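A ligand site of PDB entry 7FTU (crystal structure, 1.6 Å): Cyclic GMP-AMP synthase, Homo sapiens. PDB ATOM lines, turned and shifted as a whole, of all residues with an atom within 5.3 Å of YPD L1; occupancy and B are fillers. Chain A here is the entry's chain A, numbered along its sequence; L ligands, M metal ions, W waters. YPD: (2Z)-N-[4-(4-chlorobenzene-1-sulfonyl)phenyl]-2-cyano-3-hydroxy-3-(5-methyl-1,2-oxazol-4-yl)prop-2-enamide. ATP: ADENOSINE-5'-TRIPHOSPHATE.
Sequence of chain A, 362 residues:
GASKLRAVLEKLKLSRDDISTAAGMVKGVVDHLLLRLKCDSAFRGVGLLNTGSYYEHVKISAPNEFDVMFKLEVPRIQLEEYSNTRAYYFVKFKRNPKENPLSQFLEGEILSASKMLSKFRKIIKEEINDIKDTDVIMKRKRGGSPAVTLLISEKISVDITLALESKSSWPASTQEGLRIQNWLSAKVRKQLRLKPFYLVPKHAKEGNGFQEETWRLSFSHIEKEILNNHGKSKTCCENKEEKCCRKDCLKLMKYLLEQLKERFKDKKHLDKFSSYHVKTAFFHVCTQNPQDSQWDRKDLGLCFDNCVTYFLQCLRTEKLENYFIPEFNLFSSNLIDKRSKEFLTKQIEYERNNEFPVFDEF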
ATOM      1  N   THR A  51     -16.472 -19.584  -2.212  1.00  0.00           N
ATOM      2  CA  THR A  51     -15.440 -19.431  -3.229  1.00  0.00           C
ATOM      3  C   THR A  51     -14.878 -18.013  -3.213  1.00  0.00           C
ATOM      4  O   THR A  51     -15.322 -17.158  -2.449  1.00  0.00           O
ATOM      5  CB  THR A  51     -16.013 -19.760  -4.607  1.00  0.00           C
ATOM      6  OG1 THR A  51     -17.051 -18.812  -4.867  1.00  0.00           O
ATOM      7  CG2 THR A  51     -16.566 -21.173  -4.690  1.00  0.00           C
ATOM      8  N   ASP A  67     -18.075 -14.261  -2.297  1.00  0.00           N
ATOM      9  CA  ASP A  67     -18.580 -14.983  -3.437  1.00  0.00           C
ATOM     10  C   ASP A  67     -19.012 -16.365  -2.951  1.00  0.00           C
ATOM     11  O   ASP A  67     -18.273 -17.011  -2.197  1.00  0.00           O
ATOM     12  CB  ASP A  67     -17.523 -15.072  -4.540  1.00  0.00           C
ATOM     13  CG  ASP A  67     -17.000 -13.716  -4.952  1.00  0.00           C
ATOM     14  OD1 ASP A  67     -17.671 -13.050  -5.785  1.00  0.00           O
ATOM     15  OD2 ASP A  67     -15.901 -13.329  -4.437  1.00  0.00           O
ATOM     16  N   VAL A  68     -20.205 -16.789  -3.391  1.00  0.00           N
ATOM     17  CA  VAL A  68     -20.735 -18.087  -3.062  1.00  0.00           C
ATOM     18  C   VAL A  68     -21.443 -18.695  -4.282  1.00  0.00           C
ATOM     19  O   VAL A  68     -22.029 -17.998  -5.101  1.00  0.00           O
ATOM     20  CB  VAL A  68     -21.675 -18.042  -1.840  1.00  0.00           C
ATOM     21  CG1 VAL A  68     -20.946 -17.569  -0.581  1.00  0.00           C
ATOM     22  CG2 VAL A  68     -22.932 -17.196  -2.086  1.00  0.00           C
ATOM     23  N   MET A  69     -21.292 -20.011  -4.412  1.00  0.00           N
ATOM     24  CA  MET A  69     -22.055 -20.786  -5.357  1.00  0.00           C
ATOM     25  C   MET A  69     -23.194 -21.426  -4.572  1.00  0.00           C
ATOM     26  O   MET A  69     -22.965 -21.998  -3.506  1.00  0.00           O
ATOM     27  CB  MET A  69     -21.187 -21.864  -5.998  1.00  0.00           C
ATOM     28  CG  MET A  69     -19.942 -21.298  -6.679  1.00  0.00           C
ATOM     29  SD  MET A  69     -18.866 -22.529  -7.479  1.00  0.00           S
ATOM     30  CE  MET A  69     -19.492 -24.069  -6.806  1.00  0.00           C
ATOM     31  N   ARG A 142     -26.415  -7.253 -13.861  1.00  0.00           N
ATOM     32  CA  ARG A 142     -25.435  -6.966 -14.890  1.00  0.00           C
ATOM     33  C   ARG A 142     -25.641  -7.940 -16.051  1.00  0.00           C
ATOM     34  O   ARG A 142     -25.632  -9.147 -15.849  1.00  0.00           O
ATOM     35  CB  ARG A 142     -23.985  -7.063 -14.401  1.00  0.00           C
ATOM     36  CG  ARG A 142     -22.983  -6.743 -15.495  1.00  0.00           C
ATOM     37  CD  ARG A 142     -21.553  -6.539 -15.060  1.00  0.00           C
ATOM     38  NE  ARG A 142     -20.755  -6.236 -16.235  1.00  0.00           N
ATOM     39  CZ  ARG A 142     -19.585  -5.588 -16.232  1.00  0.00           C
ATOM     40  NH1 ARG A 142     -19.042  -5.187 -15.097  1.00  0.00           N
ATOM     41  NH2 ARG A 142     -18.966  -5.348 -17.378  1.00  0.00           N
ATOM     42  N   GLY A 143     -25.792  -7.380 -17.262  1.00  0.00           N
ATOM     43  CA  GLY A 143     -26.004  -8.167 -18.460  1.00  0.00           C
ATOM     44  C   GLY A 143     -24.956  -9.267 -18.614  1.00  0.00           C
ATOM     45  O   GLY A 143     -23.763  -8.996 -18.609  1.00  0.00           O
ATOM     46  N   GLY A 144     -25.434 -10.515 -18.712  1.00  0.00           N
ATOM     47  CA  GLY A 144     -24.586 -11.640 -19.077  1.00  0.00           C
ATOM     48  C   GLY A 144     -23.796 -12.196 -17.895  1.00  0.00           C
ATOM     49  O   GLY A 144     -23.111 -13.208 -18.048  1.00  0.00           O
ATOM     50  N   SER A 145     -23.880 -11.533 -16.728  1.00  0.00           N
ATOM     51  CA  SER A 145     -23.224 -12.000 -15.524  1.00  0.00           C
ATOM     52  C   SER A 145     -23.995 -13.174 -14.920  1.00  0.00           C
ATOM     53  O   SER A 145     -25.223 -13.232 -15.000  1.00  0.00           O
ATOM     54  CB  SER A 145     -23.070 -10.886 -14.509  1.00  0.00           C
ATOM     55  OG  SER A 145     -22.672 -11.399 -13.243  1.00  0.00           O
ATOM     56  N   PRO A 146     -23.292 -14.136 -14.284  1.00  0.00           N
ATOM     57  CA  PRO A 146     -23.960 -15.209 -13.550  1.00  0.00           C
ATOM     58  C   PRO A 146     -24.383 -14.780 -12.147  1.00  0.00           C
ATOM     59  O   PRO A 146     -25.155 -15.482 -11.509  1.00  0.00           O
ATOM     60  CB  PRO A 146     -22.869 -16.286 -13.493  1.00  0.00           C
ATOM     61  CG  PRO A 146     -21.591 -15.487 -13.380  1.00  0.00           C
ATOM     62  CD  PRO A 146     -21.831 -14.253 -14.230  1.00  0.00           C
ATOM     63  N   ALA A 147     -23.867 -13.630 -11.695  1.00  0.00           N
ATOM     64  CA  ALA A 147     -23.982 -13.212 -10.311  1.00  0.00           C
ATOM     65  C   ALA A 147     -25.351 -12.597 -10.057  1.00  0.00           C
ATOM     66  O   ALA A 147     -25.860 -11.847 -10.882  1.00  0.00           O
ATOM     67  CB  ALA A 147     -22.891 -12.223  -9.988  1.00  0.00           C
ATOM     68  N   ASP A 159     -21.780 -11.770  -3.950  1.00  0.00           N
ATOM     69  CA  ASP A 159     -22.135 -12.330  -5.245  1.00  0.00           C
ATOM     70  C   ASP A 159     -22.582 -13.756  -5.020  1.00  0.00           C
ATOM     71  O   ASP A 159     -21.830 -14.571  -4.485  1.00  0.00           O
ATOM     72  CB  ASP A 159     -20.958 -12.306  -6.228  1.00  0.00           C
ATOM     73  CG  ASP A 159     -20.507 -10.921  -6.669  1.00  0.00           C
ATOM     74  OD1 ASP A 159     -21.349  -9.973  -6.594  1.00  0.00           O
ATOM     75  OD2 ASP A 159     -19.312 -10.806  -7.057  1.00  0.00           O
ATOM     76  N   ILE A 160     -23.822 -14.032  -5.432  1.00  0.00           N
ATOM     77  CA  ILE A 160     -24.375 -15.378  -5.445  1.00  0.00           C
ATOM     78  C   ILE A 160     -24.521 -15.799  -6.905  1.00  0.00           C
ATOM     79  O   ILE A 160     -25.202 -15.134  -7.680  1.00  0.00           O
ATOM     80  CB  ILE A 160     -25.730 -15.427  -4.723  1.00  0.00           C
ATOM     81  CG1 ILE A 160     -25.665 -14.850  -3.306  1.00  0.00           C
ATOM     82  CG2 ILE A 160     -26.270 -16.849  -4.722  1.00  0.00           C
ATOM     83  CD1 ILE A 160     -27.009 -14.696  -2.638  1.00  0.00           C
ATOM     84  N   THR A 161     -23.894 -16.919  -7.255  1.00  0.00           N
ATOM     85  CA  THR A 161     -24.143 -17.550  -8.536  1.00  0.00           C
ATOM     86  C   THR A 161     -24.844 -18.869  -8.283  1.00  0.00           C
ATOM     87  O   THR A 161     -24.443 -19.646  -7.410  1.00  0.00           O
ATOM     88  CB  THR A 161     -22.859 -17.739  -9.362  1.00  0.00           C
ATOM     89  OG1 THR A 161     -23.256 -18.233 -10.650  1.00  0.00           O
ATOM     90  CG2 THR A 161     -21.866 -18.690  -8.731  1.00  0.00           C
ATOM     91  N   VAL A 200     -22.241 -22.170 -14.630  1.00  0.00           N
ATOM     92  CA  VAL A 200     -22.930 -20.991 -14.125  1.00  0.00           C
ATOM     93  C   VAL A 200     -23.598 -20.289 -15.305  1.00  0.00           C
ATOM     94  O   VAL A 200     -23.115 -20.383 -16.448  1.00  0.00           O
ATOM     95  CB  VAL A 200     -21.980 -20.038 -13.364  1.00  0.00           C
ATOM     96  CG1 VAL A 200     -21.343 -20.740 -12.179  1.00  0.00           C
ATOM     97  CG2 VAL A 200     -20.916 -19.452 -14.281  1.00  0.00           C
ATOM     98  N   LYS A 202     -23.465 -17.610 -16.907  1.00  0.00           N
ATOM     99  CA  LYS A 202     -22.794 -16.546 -17.645  1.00  0.00           C
ATOM    100  C   LYS A 202     -22.992 -16.866 -19.122  1.00  0.00           C
ATOM    101  O   LYS A 202     -22.627 -17.946 -19.583  1.00  0.00           O
ATOM    102  CB  LYS A 202     -21.313 -16.471 -17.229  1.00  0.00           C
ATOM    103  CG  LYS A 202     -20.612 -15.150 -17.527  1.00  0.00           C
ATOM    104  CD  LYS A 202     -19.869 -15.102 -18.829  1.00  0.00           C
ATOM    105  CE  LYS A 202     -19.443 -13.703 -19.225  1.00  0.00           C
ATOM    106  NZ  LYS A 202     -20.521 -13.009 -19.958  1.00  0.00           N
ATOM    107  N   ARG A 216     -21.565 -21.308 -18.668  1.00  0.00           N
ATOM    108  CA  ARG A 216     -20.111 -21.328 -18.722  1.00  0.00           C
ATOM    109  C   ARG A 216     -19.536 -22.202 -17.606  1.00  0.00           C
ATOM    110  O   ARG A 216     -20.058 -22.214 -16.491  1.00  0.00           O
ATOM    111  CB  ARG A 216     -19.526 -19.922 -18.590  1.00  0.00           C
ATOM    112  CG  ARG A 216     -18.143 -19.798 -19.219  1.00  0.00           C
ATOM    113  CD  ARG A 216     -17.281 -18.725 -18.588  1.00  0.00           C
ATOM    114  NE  ARG A 216     -17.023 -19.096 -17.212  1.00  0.00           N
ATOM    115  CZ  ARG A 216     -17.266 -18.323 -16.157  1.00  0.00           C
ATOM    116  NH1 ARG A 216     -17.221 -18.846 -14.945  1.00  0.00           N
ATOM    117  NH2 ARG A 216     -17.608 -17.058 -16.311  1.00  0.00           N
ATOM    118  N   LEU A 217     -18.450 -22.917 -17.905  1.00  0.00           N
ATOM    119  CA  LEU A 217     -17.786 -23.735 -16.899  1.00  0.00           C
ATOM    120  C   LEU A 217     -17.216 -22.850 -15.796  1.00  0.00           C
ATOM    121  O   LEU A 217     -16.768 -21.727 -16.057  1.00  0.00           O
ATOM    122  CB  LEU A 217     -16.645 -24.545 -17.542  1.00  0.00           C
ATOM    123  CG  LEU A 217     -17.072 -25.659 -18.481  1.00  0.00           C
ATOM    124  CD1 LEU A 217     -15.866 -26.204 -19.233  1.00  0.00           C
ATOM    125  CD2 LEU A 217     -17.748 -26.773 -17.722  1.00  0.00           C
ATOM    126  N   SER A 218     -17.230 -23.383 -14.580  1.00  0.00           N
ATOM    127  CA  SER A 218     -16.625 -22.748 -13.421  1.00  0.00           C
ATOM    128  C   SER A 218     -15.816 -23.786 -12.636  1.00  0.00           C
ATOM    129  O   SER A 218     -16.287 -24.901 -12.402  1.00  0.00           O
ATOM    130  CB  SER A 218     -17.657 -22.092 -12.557  1.00  0.00           C
ATOM    131  OG  SER A 218     -17.093 -21.661 -11.317  1.00  0.00           O
ATOM    132  N   SER A 220     -14.204 -22.650  -9.640  1.00  0.00           N
ATOM    133  CA  SER A 220     -13.898 -21.828  -8.472  1.00  0.00           C
ATOM    134  C   SER A 220     -13.499 -22.676  -7.271  1.00  0.00           C
ATOM    135  O   SER A 220     -12.717 -22.225  -6.420  1.00  0.00           O
ATOM    136  CB  SER A 220     -15.069 -20.944  -8.117  1.00  0.00           C
ATOM    137  OG  SER A 220     -15.331 -20.004  -9.154  1.00  0.00           O
ATOM    138  N   LYS A 261      -7.084   0.991 -11.951  1.00  0.00           N
ATOM    139  CA  LYS A 261      -8.484   1.224 -12.295  1.00  0.00           C
ATOM    140  C   LYS A 261      -9.021   2.479 -11.589  1.00  0.00           C
ATOM    141  O   LYS A 261      -9.697   3.289 -12.219  1.00  0.00           O
ATOM    142  CB  LYS A 261      -9.314  -0.021 -11.971  1.00  0.00           C
ATOM    143  CG  LYS A 261      -9.064  -1.186 -12.927  1.00  0.00           C
ATOM    144  CD  LYS A 261      -9.637  -2.520 -12.474  1.00  0.00           C
ATOM    145  CE  LYS A 261     -11.142  -2.568 -12.414  1.00  0.00           C
ATOM    146  NZ  LYS A 261     -11.753  -2.475 -13.756  1.00  0.00           N
ATOM    147  N   ASP A 271     -11.938  -0.436 -17.731  1.00  0.00           N
ATOM    148  CA  ASP A 271     -13.194  -1.028 -17.279  1.00  0.00           C
ATOM    149  C   ASP A 271     -13.278  -2.522 -17.604  1.00  0.00           C
ATOM    150  O   ASP A 271     -13.960  -3.246 -16.900  1.00  0.00           O
ATOM    151  CB  ASP A 271     -14.398  -0.242 -17.805  1.00  0.00           C
ATOM    152  CG  ASP A 271     -14.682   1.041 -17.032  1.00  0.00           C
ATOM    153  OD1 ASP A 271     -13.901   1.358 -16.116  1.00  0.00           O
ATOM    154  OD2 ASP A 271     -15.678   1.724 -17.349  1.00  0.00           O
ATOM    155  N   LYS A 272     -12.591  -3.006 -18.643  1.00  0.00           N
ATOM    156  CA  LYS A 272     -12.771  -4.390 -19.066  1.00  0.00           C
ATOM    157  C   LYS A 272     -11.831  -5.344 -18.314  1.00  0.00           C
ATOM    158  O   LYS A 272     -11.932  -6.556 -18.474  1.00  0.00           O
ATOM    159  CB  LYS A 272     -12.577  -4.454 -20.582  1.00  0.00           C
ATOM    160  CG  LYS A 272     -13.751  -3.955 -21.404  1.00  0.00           C
ATOM    161  CD  LYS A 272     -14.732  -5.058 -21.758  1.00  0.00           C
ATOM    162  CE  LYS A 272     -15.870  -4.606 -22.644  1.00  0.00           C
ATOM    163  NZ  LYS A 272     -16.939  -3.963 -21.861  1.00  0.00           N
ATOM    164  N   PHE A 273     -10.948  -4.815 -17.460  1.00  0.00           N
ATOM    165  CA  PHE A 273     -10.020  -5.665 -16.707  1.00  0.00           C
ATOM    166  C   PHE A 273     -10.573  -5.957 -15.313  1.00  0.00           C
ATOM    167  O   PHE A 273     -11.194  -5.100 -14.692  1.00  0.00           O
ATOM    168  CB  PHE A 273      -8.632  -5.011 -16.655  1.00  0.00           C
ATOM    169  CG  PHE A 273      -8.005  -4.857 -18.020  1.00  0.00           C
ATOM    170  CD1 PHE A 273      -7.526  -5.962 -18.705  1.00  0.00           C
ATOM    171  CD2 PHE A 273      -7.947  -3.615 -18.637  1.00  0.00           C
ATOM    172  CE1 PHE A 273      -6.979  -5.823 -19.963  1.00  0.00           C
ATOM    173  CE2 PHE A 273      -7.378  -3.479 -19.899  1.00  0.00           C
ATOM    174  CZ  PHE A 273      -6.908  -4.587 -20.562  1.00  0.00           C
ATOM    175  N   SER A 274     -10.301  -7.178 -14.839  1.00  0.00           N
ATOM    176  CA  SER A 274     -10.818  -7.646 -13.556  1.00  0.00           C
ATOM    177  C   SER A 274      -9.759  -8.446 -12.797  1.00  0.00           C
ATOM    178  O   SER A 274      -8.756  -8.918 -13.353  1.00  0.00           O
ATOM    179  CB  SER A 274     -12.027  -8.498 -13.787  1.00  0.00           C
ATOM    180  OG  SER A 274     -11.639  -9.824 -14.142  1.00  0.00           O
HETATM  181  C13 YPD L   1     -20.167 -15.567  -7.286  1.00  0.00           C
HETATM  182  C15 YPD L   1     -18.425 -13.480 -13.421  1.00  0.00           C
HETATM  183  C16 YPD L   1     -19.053 -12.289 -13.090  1.00  0.00           C
HETATM  184  C17 YPD L   1     -19.190 -11.281 -14.030  1.00  0.00           C
HETATM  185  C18 YPD L   1     -18.678 -11.467 -15.306  1.00  0.00           C
HETATM  186  C19 YPD L   1     -18.033 -12.642 -15.655  1.00  0.00           C
HETATM  187  C20 YPD L   1     -17.907 -13.649 -14.701  1.00  0.00           C
HETATM  188  C22 YPD L   1     -17.551  -9.042 -16.214  1.00  0.00           C
HETATM  189  C23 YPD L   1     -16.480  -8.981 -17.092  1.00  0.00           C
HETATM  190  C24 YPD L   1     -15.454  -8.084 -16.853  1.00  0.00           C
HETATM  191  C25 YPD L   1     -15.516  -7.257 -15.752  1.00  0.00           C
HETATM  192  C26 YPD L   1     -16.577  -7.314 -14.874  1.00  0.00           C
HETATM  193  C27 YPD L   1     -17.602  -8.216 -15.104  1.00  0.00           C
HETATM  194  C1  YPD L   1     -18.105 -15.807 -12.526  1.00  0.00           C
HETATM  195  O2  YPD L   1     -17.808 -16.351 -13.594  1.00  0.00           O
HETATM  196  C3  YPD L   1     -18.200 -16.618 -11.308  1.00  0.00           C
HETATM  197  C4  YPD L   1     -17.992 -18.015 -11.455  1.00  0.00           C
HETATM  198  N5  YPD L   1     -17.820 -19.127 -11.616  1.00  0.00           N
HETATM  199  C6  YPD L   1     -18.460 -16.133 -10.037  1.00  0.00           C
HETATM  200  O7  YPD L   1     -18.658 -14.839  -9.832  1.00  0.00           O
HETATM  201  C8  YPD L   1     -18.519 -16.929  -8.805  1.00  0.00           C
HETATM  202  C9  YPD L   1     -19.237 -16.651  -7.676  1.00  0.00           C
HETATM  203  O10 YPD L   1     -19.028 -17.616  -6.770  1.00  0.00           O
HETATM  204  N11 YPD L   1     -18.126 -18.571  -7.293  1.00  0.00           N
HETATM  205  C12 YPD L   1     -17.844 -18.125  -8.483  1.00  0.00           C
HETATM  206  N14 YPD L   1     -18.319 -14.458 -12.403  1.00  0.00           N
HETATM  207  S21 YPD L   1     -18.867 -10.183 -16.503  1.00  0.00           S
HETATM  208 CL28 YPD L   1     -14.239  -6.124 -15.450  1.00  0.00          CL
HETATM  209  O29 YPD L   1     -18.662 -10.759 -17.813  1.00  0.00           O
HETATM  210  O30 YPD L   1     -20.106  -9.514 -16.229  1.00  0.00           O
HETATM  211  PG  ATP L   2     -11.825 -10.175  -5.495  1.00  0.00           P
HETATM  212  O1G ATP L   2     -13.294 -10.415  -5.188  1.00  0.00           O
HETATM  213  O2G ATP L   2     -11.564  -9.227  -6.609  1.00  0.00           O
HETATM  214  O3G ATP L   2     -10.966  -9.917  -4.290  1.00  0.00           O
HETATM  215  PB  ATP L   2     -12.214 -12.882  -6.441  1.00  0.00           P
HETATM  216  O1B ATP L   2     -11.329 -14.020  -6.887  1.00  0.00           O
HETATM  217  O2B ATP L   2     -13.216 -13.137  -5.335  1.00  0.00           O
HETATM  218  O3B ATP L   2     -11.337 -11.614  -6.074  1.00  0.00           O
HETATM  219  PA  ATP L   2     -14.581 -12.160  -8.010  1.00  0.00           P
HETATM  220  O1A ATP L   2     -14.648 -11.169  -9.130  1.00  0.00           O
HETATM  221  O2A ATP L   2     -15.386 -11.878  -6.751  1.00  0.00           O
HETATM  222  O3A ATP L   2     -13.023 -12.296  -7.684  1.00  0.00           O
HETATM  223  O5' ATP L   2     -14.916 -13.615  -8.561  1.00  0.00           O
HETATM  224  C5' ATP L   2     -15.132 -14.700  -7.641  1.00  0.00           C
HETATM  225  C4' ATP L   2     -14.704 -15.976  -8.307  1.00  0.00           C
HETATM  226  O4' ATP L   2     -15.483 -16.156  -9.517  1.00  0.00           O
HETATM  227  C3' ATP L   2     -13.263 -16.041  -8.806  1.00  0.00           C
HETATM  228  O3' ATP L   2     -12.365 -16.305  -7.737  1.00  0.00           O
HETATM  229  C2' ATP L   2     -13.371 -17.169  -9.836  1.00  0.00           C
HETATM  230  O2' ATP L   2     -13.344 -18.448  -9.252  1.00  0.00           O
HETATM  231  C1' ATP L   2     -14.739 -16.894 -10.460  1.00  0.00           C
HETATM  232  N9  ATP L   2     -14.679 -16.103 -11.684  1.00  0.00           N
HETATM  233  C8  ATP L   2     -14.770 -14.738 -11.789  1.00  0.00           C
HETATM  234  N7  ATP L   2     -14.673 -14.333 -13.030  1.00  0.00           N
HETATM  235  C5  ATP L   2     -14.500 -15.494 -13.766  1.00  0.00           C
HETATM  236  C6  ATP L   2     -14.329 -15.726 -15.151  1.00  0.00           C
HETATM  237  N6  ATP L   2     -14.288 -14.753 -16.057  1.00  0.00           N
HETATM  238  N1  ATP L   2     -14.186 -17.004 -15.556  1.00  0.00           N
HETATM  239  C2  ATP L   2     -14.186 -17.974 -14.632  1.00  0.00           C
HETATM  240  N3  ATP L   2     -14.336 -17.879 -13.311  1.00  0.00           N
HETATM  241  C4  ATP L   2     -14.491 -16.593 -12.946  1.00  0.00           C
HETATM  242 MG    MG M   1     -17.384 -11.414  -6.891  1.00  0.00          MG
HETATM  243  O   HOH W   1     -17.794 -12.524  -8.551  1.00  0.00           O
HETATM  244  O   HOH W   2     -14.054  -6.057 -12.287  1.00  0.00           O
HETATM  245  O   HOH W   3     -16.569 -11.189 -11.141  1.00  0.00           O
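The backbone NH (N) of Thr 51 sits at hydrogen-bond distance from the backbone carbonyl oxygen (O) of Asp 67, at 3.1 Å. N of Arg 216 sits at hydrogen-bond distance from O of Val 200 (2.9 Å). The backbone carbonyl oxygen (O) of Phe 273 sits at hydrogen-bond distance from the side-chain amino group (NZ) of Lys 261. The side-chain amino group of Lys 202 sits close to the backbone carbonyl oxygen of Gly 144 (3.2 Å). The backbone NH of Val 68 is in hydrogen-bond range of the backbone carbonyl oxygen of Asp 159 (3.0 Å). N of Thr 161 sits at hydrogen-bond distance from O of Val 68, 3.0 Å away. OG1 of Thr 161 is in hydrogen-bond range of O of Pro 146, at 3.5 Å. The side-chain hydroxyl (OG) of Ser 145 sits at hydrogen-bond distance from the backbone NH (N) of Ala 147, 3.0 Å away.
OG of Ser 218 sits at hydrogen-bond distance from N5 of YPD L1, 2.7 Å away. OG1 of Thr 51 lies within hydrogen-bond range of N11 of YPD L1, at 2.7 Å. NH2 of Arg 216 sits at hydrogen-bond distance from O2 of YPD L1, 2.8 Å away. O30 of YPD L1 sits at hydrogen-bond distance from NE of Arg 142 (3.3 Å). The guanidinium group (NH1) of Arg 216 sits close to a nitrogen (N3) of ATP L2, 3.5 Å away. O2' of ATP L2 sits at hydrogen-bond distance from OG of Ser 220, 2.5 Å away.
O of Val 68 lies close to O10 of YPD L1, 3.5 Å away. Merely in contact with YPD L1: Ser 220 (3.2 Å), Asp 271 (3.2 Å), Phe 273 (3.3 Å), Met 69 (3.3 Å), Lys 202 (3.4 Å), Asp 159 (3.4 Å), Thr 161 (3.5 Å), Pro 146 (3.6 Å), Ser 145 (3.6 Å), Ser 274 (3.6 Å), Asp 67 (3.7 Å), Lys 272 (3.8 Å) and Val 200 (3.9 Å). Hydrophobic or aromatic side chains within 4 Å of YPD L1: Met 69, Pro 146 and Val 200.
O7 of YPD L1 sits close to O4' of ATP L2 (3.5 Å).
Water W1 lies within hydrogen-bond range of an oxygen (O7) of YPD L1 (2.8 Å) and an oxygen (O5') of ATP L2 (3.1 Å).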
